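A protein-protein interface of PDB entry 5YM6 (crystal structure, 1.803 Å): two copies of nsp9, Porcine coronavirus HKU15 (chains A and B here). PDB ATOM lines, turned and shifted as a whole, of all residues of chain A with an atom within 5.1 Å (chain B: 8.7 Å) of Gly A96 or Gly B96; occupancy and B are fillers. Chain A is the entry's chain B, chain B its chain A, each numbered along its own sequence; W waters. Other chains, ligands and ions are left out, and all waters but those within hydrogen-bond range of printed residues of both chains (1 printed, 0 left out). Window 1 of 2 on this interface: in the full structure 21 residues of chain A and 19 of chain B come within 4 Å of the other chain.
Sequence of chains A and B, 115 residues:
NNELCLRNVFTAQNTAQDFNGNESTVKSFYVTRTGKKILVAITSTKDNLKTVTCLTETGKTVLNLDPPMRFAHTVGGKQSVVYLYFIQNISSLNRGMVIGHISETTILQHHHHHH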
ATOM      1  N   SER A  92       2.260  23.794 -12.106  1.00  0.00           N
ATOM      2  CA  SER A  92       2.415  23.264 -13.450  1.00  0.00           C
ATOM      3  C   SER A  92       1.314  23.825 -14.360  1.00  0.00           C
ATOM      4  O   SER A  92       1.541  24.019 -15.551  1.00  0.00           O
ATOM      5  CB  SER A  92       2.382  21.732 -13.443  1.00  0.00           C
ATOM      6  OG  SER A  92       3.669  21.173 -13.168  1.00  0.00           O
ATOM      7  N   LEU A  93       0.131  24.085 -13.801  1.00  0.00           N
ATOM      8  CA  LEU A  93      -0.975  24.626 -14.603  1.00  0.00           C
ATOM      9  C   LEU A  93      -0.646  26.037 -15.081  1.00  0.00           C
ATOM     10  O   LEU A  93      -0.960  26.426 -16.207  1.00  0.00           O
ATOM     11  CB  LEU A  93      -2.276  24.663 -13.813  1.00  0.00           C
ATOM     12  CG  LEU A  93      -3.561  24.980 -14.585  1.00  0.00           C
ATOM     13  CD1 LEU A  93      -4.093  23.728 -15.233  1.00  0.00           C
ATOM     14  CD2 LEU A  93      -4.623  25.552 -13.659  1.00  0.00           C
ATOM     15  N   ASN A  94      -0.021  26.809 -14.207  1.00  0.00           N
ATOM     16  CA  ASN A  94       0.310  28.179 -14.563  1.00  0.00           C
ATOM     17  C   ASN A  94       1.475  28.220 -15.533  1.00  0.00           C
ATOM     18  O   ASN A  94       1.532  29.102 -16.374  1.00  0.00           O
ATOM     19  CB  ASN A  94       0.622  29.009 -13.312  1.00  0.00           C
ATOM     20  CG  ASN A  94      -0.627  29.437 -12.575  1.00  0.00           C
ATOM     21  OD1 ASN A  94      -0.655  29.472 -11.341  1.00  0.00           O
ATOM     22  ND2 ASN A  94      -1.685  29.731 -13.324  1.00  0.00           N
ATOM     23  N   ARG A  95       2.400  27.271 -15.411  1.00  0.00           N
ATOM     24  CA  ARG A  95       3.495  27.156 -16.367  1.00  0.00           C
ATOM     25  C   ARG A  95       2.915  26.886 -17.750  1.00  0.00           C
ATOM     26  O   ARG A  95       3.333  27.496 -18.738  1.00  0.00           O
ATOM     27  CB  ARG A  95       4.479  26.055 -15.962  1.00  0.00           C
ATOM     28  CG  ARG A  95       5.277  26.386 -14.681  1.00  0.00           C
ATOM     29  CD  ARG A  95       5.885  25.145 -14.020  1.00  0.00           C
ATOM     30  NE  ARG A  95       6.997  24.572 -14.777  1.00  0.00           N
ATOM     31  CZ  ARG A  95       8.283  24.840 -14.549  1.00  0.00           C
ATOM     32  NH1 ARG A  95       9.219  24.270 -15.298  1.00  0.00           N
ATOM     33  NH2 ARG A  95       8.638  25.681 -13.577  1.00  0.00           N
ATOM     34  N   GLY A  96       1.933  25.993 -17.817  1.00  0.00           N
ATOM     35  CA  GLY A  96       1.285  25.695 -19.087  1.00  0.00           C
ATOM     36  C   GLY A  96       0.639  26.920 -19.710  1.00  0.00           C
ATOM     37  O   GLY A  96       0.731  27.123 -20.912  1.00  0.00           O
ATOM     38  N   MET A  97      -0.033  27.719 -18.895  1.00  0.00           N
ATOM     39  CA  MET A  97      -0.643  28.960 -19.383  1.00  0.00           C
ATOM     40  C   MET A  97       0.380  29.871 -20.078  1.00  0.00           C
ATOM     41  O   MET A  97       0.137  30.399 -21.170  1.00  0.00           O
ATOM     42  CB  MET A  97      -1.293  29.723 -18.224  1.00  0.00           C
ATOM     43  CG  MET A  97      -2.588  29.135 -17.695  1.00  0.00           C
ATOM     44  SD  MET A  97      -3.947  29.313 -18.850  1.00  0.00           S
ATOM     45  CE  MET A  97      -4.133  31.095 -18.950  1.00  0.00           C
ATOM     46  N   VAL A  98       1.527  30.051 -19.439  1.00  0.00           N
ATOM     47  CA  VAL A  98       2.561  30.946 -19.972  1.00  0.00           C
ATOM     48  C   VAL A  98       3.267  30.341 -21.182  1.00  0.00           C
ATOM     49  O   VAL A  98       3.509  31.030 -22.173  1.00  0.00           O
ATOM     50  CB  VAL A  98       3.571  31.310 -18.878  1.00  0.00           C
ATOM     51  CG1 VAL A  98       4.774  32.057 -19.454  1.00  0.00           C
ATOM     52  CG2 VAL A  98       2.887  32.146 -17.831  1.00  0.00           C
ATOM     53  N   ILE A  99       3.559  29.045 -21.139  1.00  0.00           N
ATOM     54  CA  ILE A  99       4.183  28.392 -22.293  1.00  0.00           C
ATOM     55  C   ILE A  99       3.276  28.485 -23.521  1.00  0.00           C
ATOM     56  O   ILE A  99       3.753  28.733 -24.630  1.00  0.00           O
ATOM     57  CB  ILE A  99       4.519  26.923 -21.996  1.00  0.00           C
ATOM     58  CG1 ILE A  99       5.641  26.851 -20.957  1.00  0.00           C
ATOM     59  CG2 ILE A  99       4.955  26.190 -23.259  1.00  0.00           C
ATOM     60  CD1 ILE A  99       5.986  25.448 -20.523  1.00  0.00           C
ATOM     61  N   GLY A 100       1.974  28.301 -23.319  1.00  0.00           N
ATOM     62  CA  GLY A 100       1.024  28.416 -24.412  1.00  0.00           C
ATOM     63  C   GLY A 100       1.010  29.815 -25.001  1.00  0.00           C
ATOM     64  O   GLY A 100       0.949  29.996 -26.221  1.00  0.00           O
ATOM     65  N   HIS A 101       1.077  30.811 -24.125  1.00  0.00           N
ATOM     66  CA  HIS A 101       1.018  32.201 -24.548  1.00  0.00           C
ATOM     67  C   HIS A 101       2.248  32.561 -25.370  1.00  0.00           C
ATOM     68  O   HIS A 101       2.133  33.158 -26.442  1.00  0.00           O
ATOM     69  CB  HIS A 101       0.887  33.120 -23.326  1.00  0.00           C
ATOM     70  CG  HIS A 101       0.703  34.566 -23.668  1.00  0.00           C
ATOM     71  ND1 HIS A 101      -0.545  35.140 -23.818  1.00  0.00           N
ATOM     72  CD2 HIS A 101       1.599  35.557 -23.873  1.00  0.00           C
ATOM     73  CE1 HIS A 101      -0.400  36.424 -24.105  1.00  0.00           C
ATOM     74  NE2 HIS A 101       0.890  36.699 -24.150  1.00  0.00           N
ATOM     75  N   ARG B   7       5.358  24.317 -27.372  1.00  0.00           N
ATOM     76  CA  ARG B   7       4.322  23.379 -27.756  1.00  0.00           C
ATOM     77  C   ARG B   7       3.194  24.137 -28.432  1.00  0.00           C
ATOM     78  O   ARG B   7       3.026  25.337 -28.218  1.00  0.00           O
ATOM     79  CB  ARG B   7       3.813  22.619 -26.537  1.00  0.00           C
ATOM     80  CG  ARG B   7       4.889  21.990 -25.668  1.00  0.00           C
ATOM     81  CD  ARG B   7       4.362  21.834 -24.250  1.00  0.00           C
ATOM     82  NE  ARG B   7       5.127  20.908 -23.415  1.00  0.00           N
ATOM     83  CZ  ARG B   7       6.279  21.203 -22.821  1.00  0.00           C
ATOM     84  NH1 ARG B   7       6.833  22.398 -22.989  1.00  0.00           N
ATOM     85  NH2 ARG B   7       6.884  20.293 -22.069  1.00  0.00           N
ATOM     86  N   VAL B   9      -1.098  24.212 -29.528  1.00  0.00           N
ATOM     87  CA  VAL B   9      -2.411  23.629 -29.318  1.00  0.00           C
ATOM     88  C   VAL B   9      -3.121  23.641 -30.653  1.00  0.00           C
ATOM     89  O   VAL B   9      -3.146  24.673 -31.343  1.00  0.00           O
ATOM     90  CB  VAL B   9      -3.239  24.393 -28.286  1.00  0.00           C
ATOM     91  CG1 VAL B   9      -4.674  23.855 -28.263  1.00  0.00           C
ATOM     92  CG2 VAL B   9      -2.573  24.303 -26.912  1.00  0.00           C
ATOM     93  N   VAL B  31      -2.447  18.942 -27.527  1.00  0.00           N
ATOM     94  CA  VAL B  31      -1.156  19.593 -27.363  1.00  0.00           C
ATOM     95  C   VAL B  31      -0.160  18.829 -28.217  1.00  0.00           C
ATOM     96  O   VAL B  31      -0.099  17.601 -28.167  1.00  0.00           O
ATOM     97  CB  VAL B  31      -0.719  19.635 -25.898  1.00  0.00           C
ATOM     98  CG1 VAL B  31       0.762  20.027 -25.780  1.00  0.00           C
ATOM     99  CG2 VAL B  31      -1.614  20.586 -25.138  1.00  0.00           C
ATOM    100  N   VAL B  40      -6.095  16.385 -24.908  1.00  0.00           N
ATOM    101  CA  VAL B  40      -6.215  16.990 -23.587  1.00  0.00           C
ATOM    102  C   VAL B  40      -7.655  17.269 -23.149  1.00  0.00           C
ATOM    103  O   VAL B  40      -7.995  17.099 -21.977  1.00  0.00           O
ATOM    104  CB  VAL B  40      -5.423  18.314 -23.543  1.00  0.00           C
ATOM    105  CG1 VAL B  40      -5.651  19.065 -22.236  1.00  0.00           C
ATOM    106  CG2 VAL B  40      -3.933  18.025 -23.752  1.00  0.00           C
ATOM    107  N   PHE B  86     -12.135  17.534 -19.580  1.00  0.00           N
ATOM    108  CA  PHE B  86     -10.743  17.129 -19.684  1.00  0.00           C
ATOM    109  C   PHE B  86     -10.627  15.608 -19.737  1.00  0.00           C
ATOM    110  O   PHE B  86     -11.435  14.882 -19.140  1.00  0.00           O
ATOM    111  CB  PHE B  86      -9.923  17.661 -18.511  1.00  0.00           C
ATOM    112  CG  PHE B  86      -9.653  19.126 -18.601  1.00  0.00           C
ATOM    113  CD1 PHE B  86      -8.745  19.597 -19.527  1.00  0.00           C
ATOM    114  CD2 PHE B  86     -10.333  20.023 -17.795  1.00  0.00           C
ATOM    115  CE1 PHE B  86      -8.488  20.947 -19.634  1.00  0.00           C
ATOM    116  CE2 PHE B  86     -10.082  21.381 -17.893  1.00  0.00           C
ATOM    117  CZ  PHE B  86      -9.162  21.841 -18.817  1.00  0.00           C
ATOM    118  N   ILE B  90      -4.859  13.735 -17.359  1.00  0.00           N
ATOM    119  CA  ILE B  90      -3.965  14.566 -18.174  1.00  0.00           C
ATOM    120  C   ILE B  90      -3.148  15.486 -17.271  1.00  0.00           C
ATOM    121  O   ILE B  90      -3.662  15.964 -16.266  1.00  0.00           O
ATOM    122  CB  ILE B  90      -4.767  15.406 -19.204  1.00  0.00           C
ATOM    123  CG1 ILE B  90      -5.118  14.552 -20.411  1.00  0.00           C
ATOM    124  CG2 ILE B  90      -3.948  16.600 -19.697  1.00  0.00           C
ATOM    125  CD1 ILE B  90      -3.913  14.169 -21.241  1.00  0.00           C
ATOM    126  N   SER B  91      -1.877  15.714 -17.612  1.00  0.00           N
ATOM    127  CA  SER B  91      -1.009  16.564 -16.801  1.00  0.00           C
ATOM    128  C   SER B  91      -1.544  17.985 -16.674  1.00  0.00           C
ATOM    129  O   SER B  91      -2.226  18.501 -17.570  1.00  0.00           O
ATOM    130  CB  SER B  91       0.412  16.590 -17.380  1.00  0.00           C
ATOM    131  OG  SER B  91       0.475  17.269 -18.626  1.00  0.00           O
ATOM    132  N   SER B  92      -1.247  18.610 -15.540  1.00  0.00           N
ATOM    133  CA  SER B  92      -1.691  19.965 -15.289  1.00  0.00           C
ATOM    134  C   SER B  92      -1.070  20.943 -16.279  1.00  0.00           C
ATOM    135  O   SER B  92      -1.705  21.927 -16.649  1.00  0.00           O
ATOM    136  CB  SER B  92      -1.365  20.392 -13.860  1.00  0.00           C
ATOM    137  OG  SER B  92      -2.344  19.923 -12.953  1.00  0.00           O
ATOM    138  N   LEU B  93       0.158  20.673 -16.708  1.00  0.00           N
ATOM    139  CA  LEU B  93       0.807  21.509 -17.711  1.00  0.00           C
ATOM    140  C   LEU B  93       0.008  21.550 -19.014  1.00  0.00           C
ATOM    141  O   LEU B  93      -0.245  22.625 -19.581  1.00  0.00           O
ATOM    142  CB  LEU B  93       2.219  21.001 -17.982  1.00  0.00           C
ATOM    143  CG  LEU B  93       3.044  21.830 -18.961  1.00  0.00           C
ATOM    144  CD1 LEU B  93       3.576  23.059 -18.263  1.00  0.00           C
ATOM    145  CD2 LEU B  93       4.189  21.009 -19.537  1.00  0.00           C
ATOM    146  N   ASN B  94      -0.404  20.375 -19.478  1.00  0.00           N
ATOM    147  CA  ASN B  94      -1.211  20.283 -20.692  1.00  0.00           C
ATOM    148  C   ASN B  94      -2.592  20.915 -20.515  1.00  0.00           C
ATOM    149  O   ASN B  94      -3.125  21.539 -21.429  1.00  0.00           O
ATOM    150  CB  ASN B  94      -1.311  18.805 -21.113  1.00  0.00           C
ATOM    151  CG  ASN B  94      -0.083  18.339 -21.874  1.00  0.00           C
ATOM    152  OD1 ASN B  94       0.646  19.149 -22.444  1.00  0.00           O
ATOM    153  ND2 ASN B  94       0.188  17.036 -21.827  1.00  0.00           N
ATOM    154  N   ARG B  95      -3.154  20.765 -19.324  1.00  0.00           N
ATOM    155  CA  ARG B  95      -4.411  21.414 -19.018  1.00  0.00           C
ATOM    156  C   ARG B  95      -4.286  22.923 -19.147  1.00  0.00           C
ATOM    157  O   ARG B  95      -5.164  23.585 -19.699  1.00  0.00           O
ATOM    158  CB  ARG B  95      -4.884  21.100 -17.602  1.00  0.00           C
ATOM    159  CG  ARG B  95      -5.481  19.739 -17.375  1.00  0.00           C
ATOM    160  CD  ARG B  95      -6.059  19.718 -15.955  1.00  0.00           C
ATOM    161  NE  ARG B  95      -6.990  18.621 -15.761  1.00  0.00           N
ATOM    162  CZ  ARG B  95      -8.129  18.721 -15.087  1.00  0.00           C
ATOM    163  NH1 ARG B  95      -8.483  19.879 -14.533  1.00  0.00           N
ATOM    164  NH2 ARG B  95      -8.906  17.661 -14.967  1.00  0.00           N
ATOM    165  N   GLY B  96      -3.200  23.450 -18.589  1.00  0.00           N
ATOM    166  CA  GLY B  96      -2.921  24.883 -18.633  1.00  0.00           C
ATOM    167  C   GLY B  96      -2.818  25.399 -20.055  1.00  0.00           C
ATOM    168  O   GLY B  96      -3.356  26.464 -20.391  1.00  0.00           O
ATOM    169  N   MET B  97      -2.128  24.641 -20.901  1.00  0.00           N
ATOM    170  CA  MET B  97      -1.981  25.012 -22.313  1.00  0.00           C
ATOM    171  C   MET B  97      -3.347  25.197 -22.971  1.00  0.00           C
ATOM    172  O   MET B  97      -3.611  26.188 -23.676  1.00  0.00           O
ATOM    173  CB  MET B  97      -1.166  23.939 -23.053  1.00  0.00           C
ATOM    174  CG  MET B  97       0.282  23.855 -22.632  1.00  0.00           C
ATOM    175  SD  MET B  97       1.299  24.868 -23.723  1.00  0.00           S
ATOM    176  CE  MET B  97       0.902  24.142 -25.302  1.00  0.00           C
ATOM    177  N   VAL B  98      -4.238  24.247 -22.721  1.00  0.00           N
ATOM    178  CA  VAL B  98      -5.535  24.274 -23.372  1.00  0.00           C
ATOM    179  C   VAL B  98      -6.441  25.366 -22.797  1.00  0.00           C
ATOM    180  O   VAL B  98      -7.166  26.032 -23.538  1.00  0.00           O
ATOM    181  CB  VAL B  98      -6.194  22.892 -23.276  1.00  0.00           C
ATOM    182  CG1 VAL B  98      -7.704  22.966 -23.532  1.00  0.00           C
ATOM    183  CG2 VAL B  98      -5.498  21.957 -24.263  1.00  0.00           C
ATOM    184  N   ILE B  99      -6.372  25.585 -21.486  1.00  0.00           N
ATOM    185  CA  ILE B  99      -7.194  26.615 -20.867  1.00  0.00           C
ATOM    186  C   ILE B  99      -6.820  27.976 -21.440  1.00  0.00           C
ATOM    187  O   ILE B  99      -7.693  28.765 -21.790  1.00  0.00           O
ATOM    188  CB  ILE B  99      -7.051  26.611 -19.333  1.00  0.00           C
ATOM    189  CG1 ILE B  99      -7.758  25.383 -18.759  1.00  0.00           C
ATOM    190  CG2 ILE B  99      -7.651  27.882 -18.716  1.00  0.00           C
ATOM    191  CD1 ILE B  99      -7.574  25.205 -17.283  1.00  0.00           C
ATOM    192  N   GLY B 100      -5.519  28.225 -21.571  1.00  0.00           N
ATOM    193  CA  GLY B 100      -5.031  29.464 -22.157  1.00  0.00           C
ATOM    194  C   GLY B 100      -5.475  29.656 -23.593  1.00  0.00           C
ATOM    195  O   GLY B 100      -5.830  30.762 -24.010  1.00  0.00           O
ATOM    196  N   HIS B 101      -5.458  28.567 -24.351  1.00  0.00           N
ATOM    197  CA  HIS B 101      -5.868  28.604 -25.746  1.00  0.00           C
ATOM    198  C   HIS B 101      -7.337  28.976 -25.888  1.00  0.00           C
ATOM    199  O   HIS B 101      -7.690  29.813 -26.717  1.00  0.00           O
ATOM    200  CB  HIS B 101      -5.604  27.258 -26.420  1.00  0.00           C
ATOM    201  CG  HIS B 101      -5.910  27.249 -27.886  1.00  0.00           C
ATOM    202  ND1 HIS B 101      -4.968  27.557 -28.844  1.00  0.00           N
ATOM    203  CD2 HIS B 101      -7.055  26.984 -28.555  1.00  0.00           C
ATOM    204  CE1 HIS B 101      -5.518  27.469 -30.042  1.00  0.00           C
ATOM    205  NE2 HIS B 101      -6.784  27.126 -29.895  1.00  0.00           N
ATOM    206  N   ILE B 102      -8.190  28.354 -25.082  1.00  0.00           N
ATOM    207  CA  ILE B 102      -9.625  28.625 -25.133  1.00  0.00           C
ATOM    208  C   ILE B 102      -9.924  30.069 -24.716  1.00  0.00           C
ATOM    209  O   ILE B 102     -10.746  30.745 -25.336  1.00  0.00           O
ATOM    210  CB  ILE B 102     -10.406  27.635 -24.247  1.00  0.00           C
ATOM    211  CG1 ILE B 102     -10.367  26.243 -24.883  1.00  0.00           C
ATOM    212  CG2 ILE B 102     -11.849  28.096 -24.048  1.00  0.00           C
ATOM    213  CD1 ILE B 102     -10.891  25.146 -24.009  1.00  0.00           C
ATOM    214  N   SER B 103      -9.229  30.544 -23.684  1.00  0.00           N
ATOM    215  CA  SER B 103      -9.374  31.919 -23.216  1.00  0.00           C
ATOM    216  C   SER B 103      -8.878  32.951 -24.227  1.00  0.00           C
ATOM    217  O   SER B 103      -9.494  34.000 -24.412  1.00  0.00           O
ATOM    218  CB  SER B 103      -8.614  32.112 -21.905  1.00  0.00           C
ATOM    219  OG  SER B 103      -9.052  31.213 -20.897  1.00  0.00           O
HETATM  220  O   HOH W   1      -0.642  22.017 -11.257  1.00  0.00           O
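Water W1 bridges the side-chain hydroxyl of Ser B92 and the backbone NH of Leu A93.
Among the printed residues, pairs that only touch across the chains: Leu A93 with Ser B92, Ser A92 with Leu B93, Gly A96 with Leu B93, Leu A93 with Gly B96, Leu A93 with Arg B95, Gly A96 with Gly B96, Arg A95 with Leu B93, Ile A99 with Met B97 and Met A97 with Ile B99.
Leu A93 touches Arg B95, and with the chains exchanged Arg A95 touches Leu B93. Gly B96 touches its own counterpart, Gly A96. Met A97 touches Ile B99, and with the chains exchanged Ile A99 touches Met B97. Met A97 touches Gly B100, and with the chains exchanged Gly A100 touches Met B97. Of the 13 pairs that touch across the chains among the printed residues, 13 have their exchanged pair printed and touching as well.
O of Ile B99 sits at hydrogen-bond distance from OG of Ser B103, 2.9 Å away.
Of chain B, only Leu B93, Gly B96 and Met B97 come within 4 Å of Gly A96. Gly B96 touches just these residues of chain A: Leu A93, Gly A96 and Met A97. Printed residues of chain B within 4 Å of Gly A100: Met B97. Of the printed residues of chain A, Ser B92 touches Leu A93. Phe B86 touches none of the printed residues of chain A. Asn A94 touches none of the printed residues of chain B. The nearest printed residue of chain A that does not touch Gly B96 is Ser A92 (5.5 Å). The nearest printed residue of chain B that does not touch Gly A100 is Arg B7 (5.3 Å).
Hydrophobic or aromatic side chains of chain B that line the printed part of chain A: Leu B93, Met B97 and Ile B99. Along chain B the printed residues that touch a printed residue of chain A span positions 92 to 100. Of the 10 printed residues of chain A, 7 touch a printed residue of chain B. Hydrophobic or aromatic side chains of chain A that line the printed part of chain B: Leu A93, Met A97 and Ile A99. Among the printed residues, 13 pairs touch across the chains.
SD of Met B97 lies within hydrogen-bond range of N of Gly A100 (3.5 Å). The backbone NH (N) of Gly B100 is in hydrogen-bond range of the side-chain sulfur (SD) of Met A97 (3.3 Å). The backbone carbonyl oxygen (O) of Gly A96 sits close to the side-chain sulfur (SD) of Met B97 (3.6 Å). The side-chain sulfur (SD) of Met A97 lies close to the backbone carbonyl oxygen (O) of Gly B96, 3.3 Å away.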
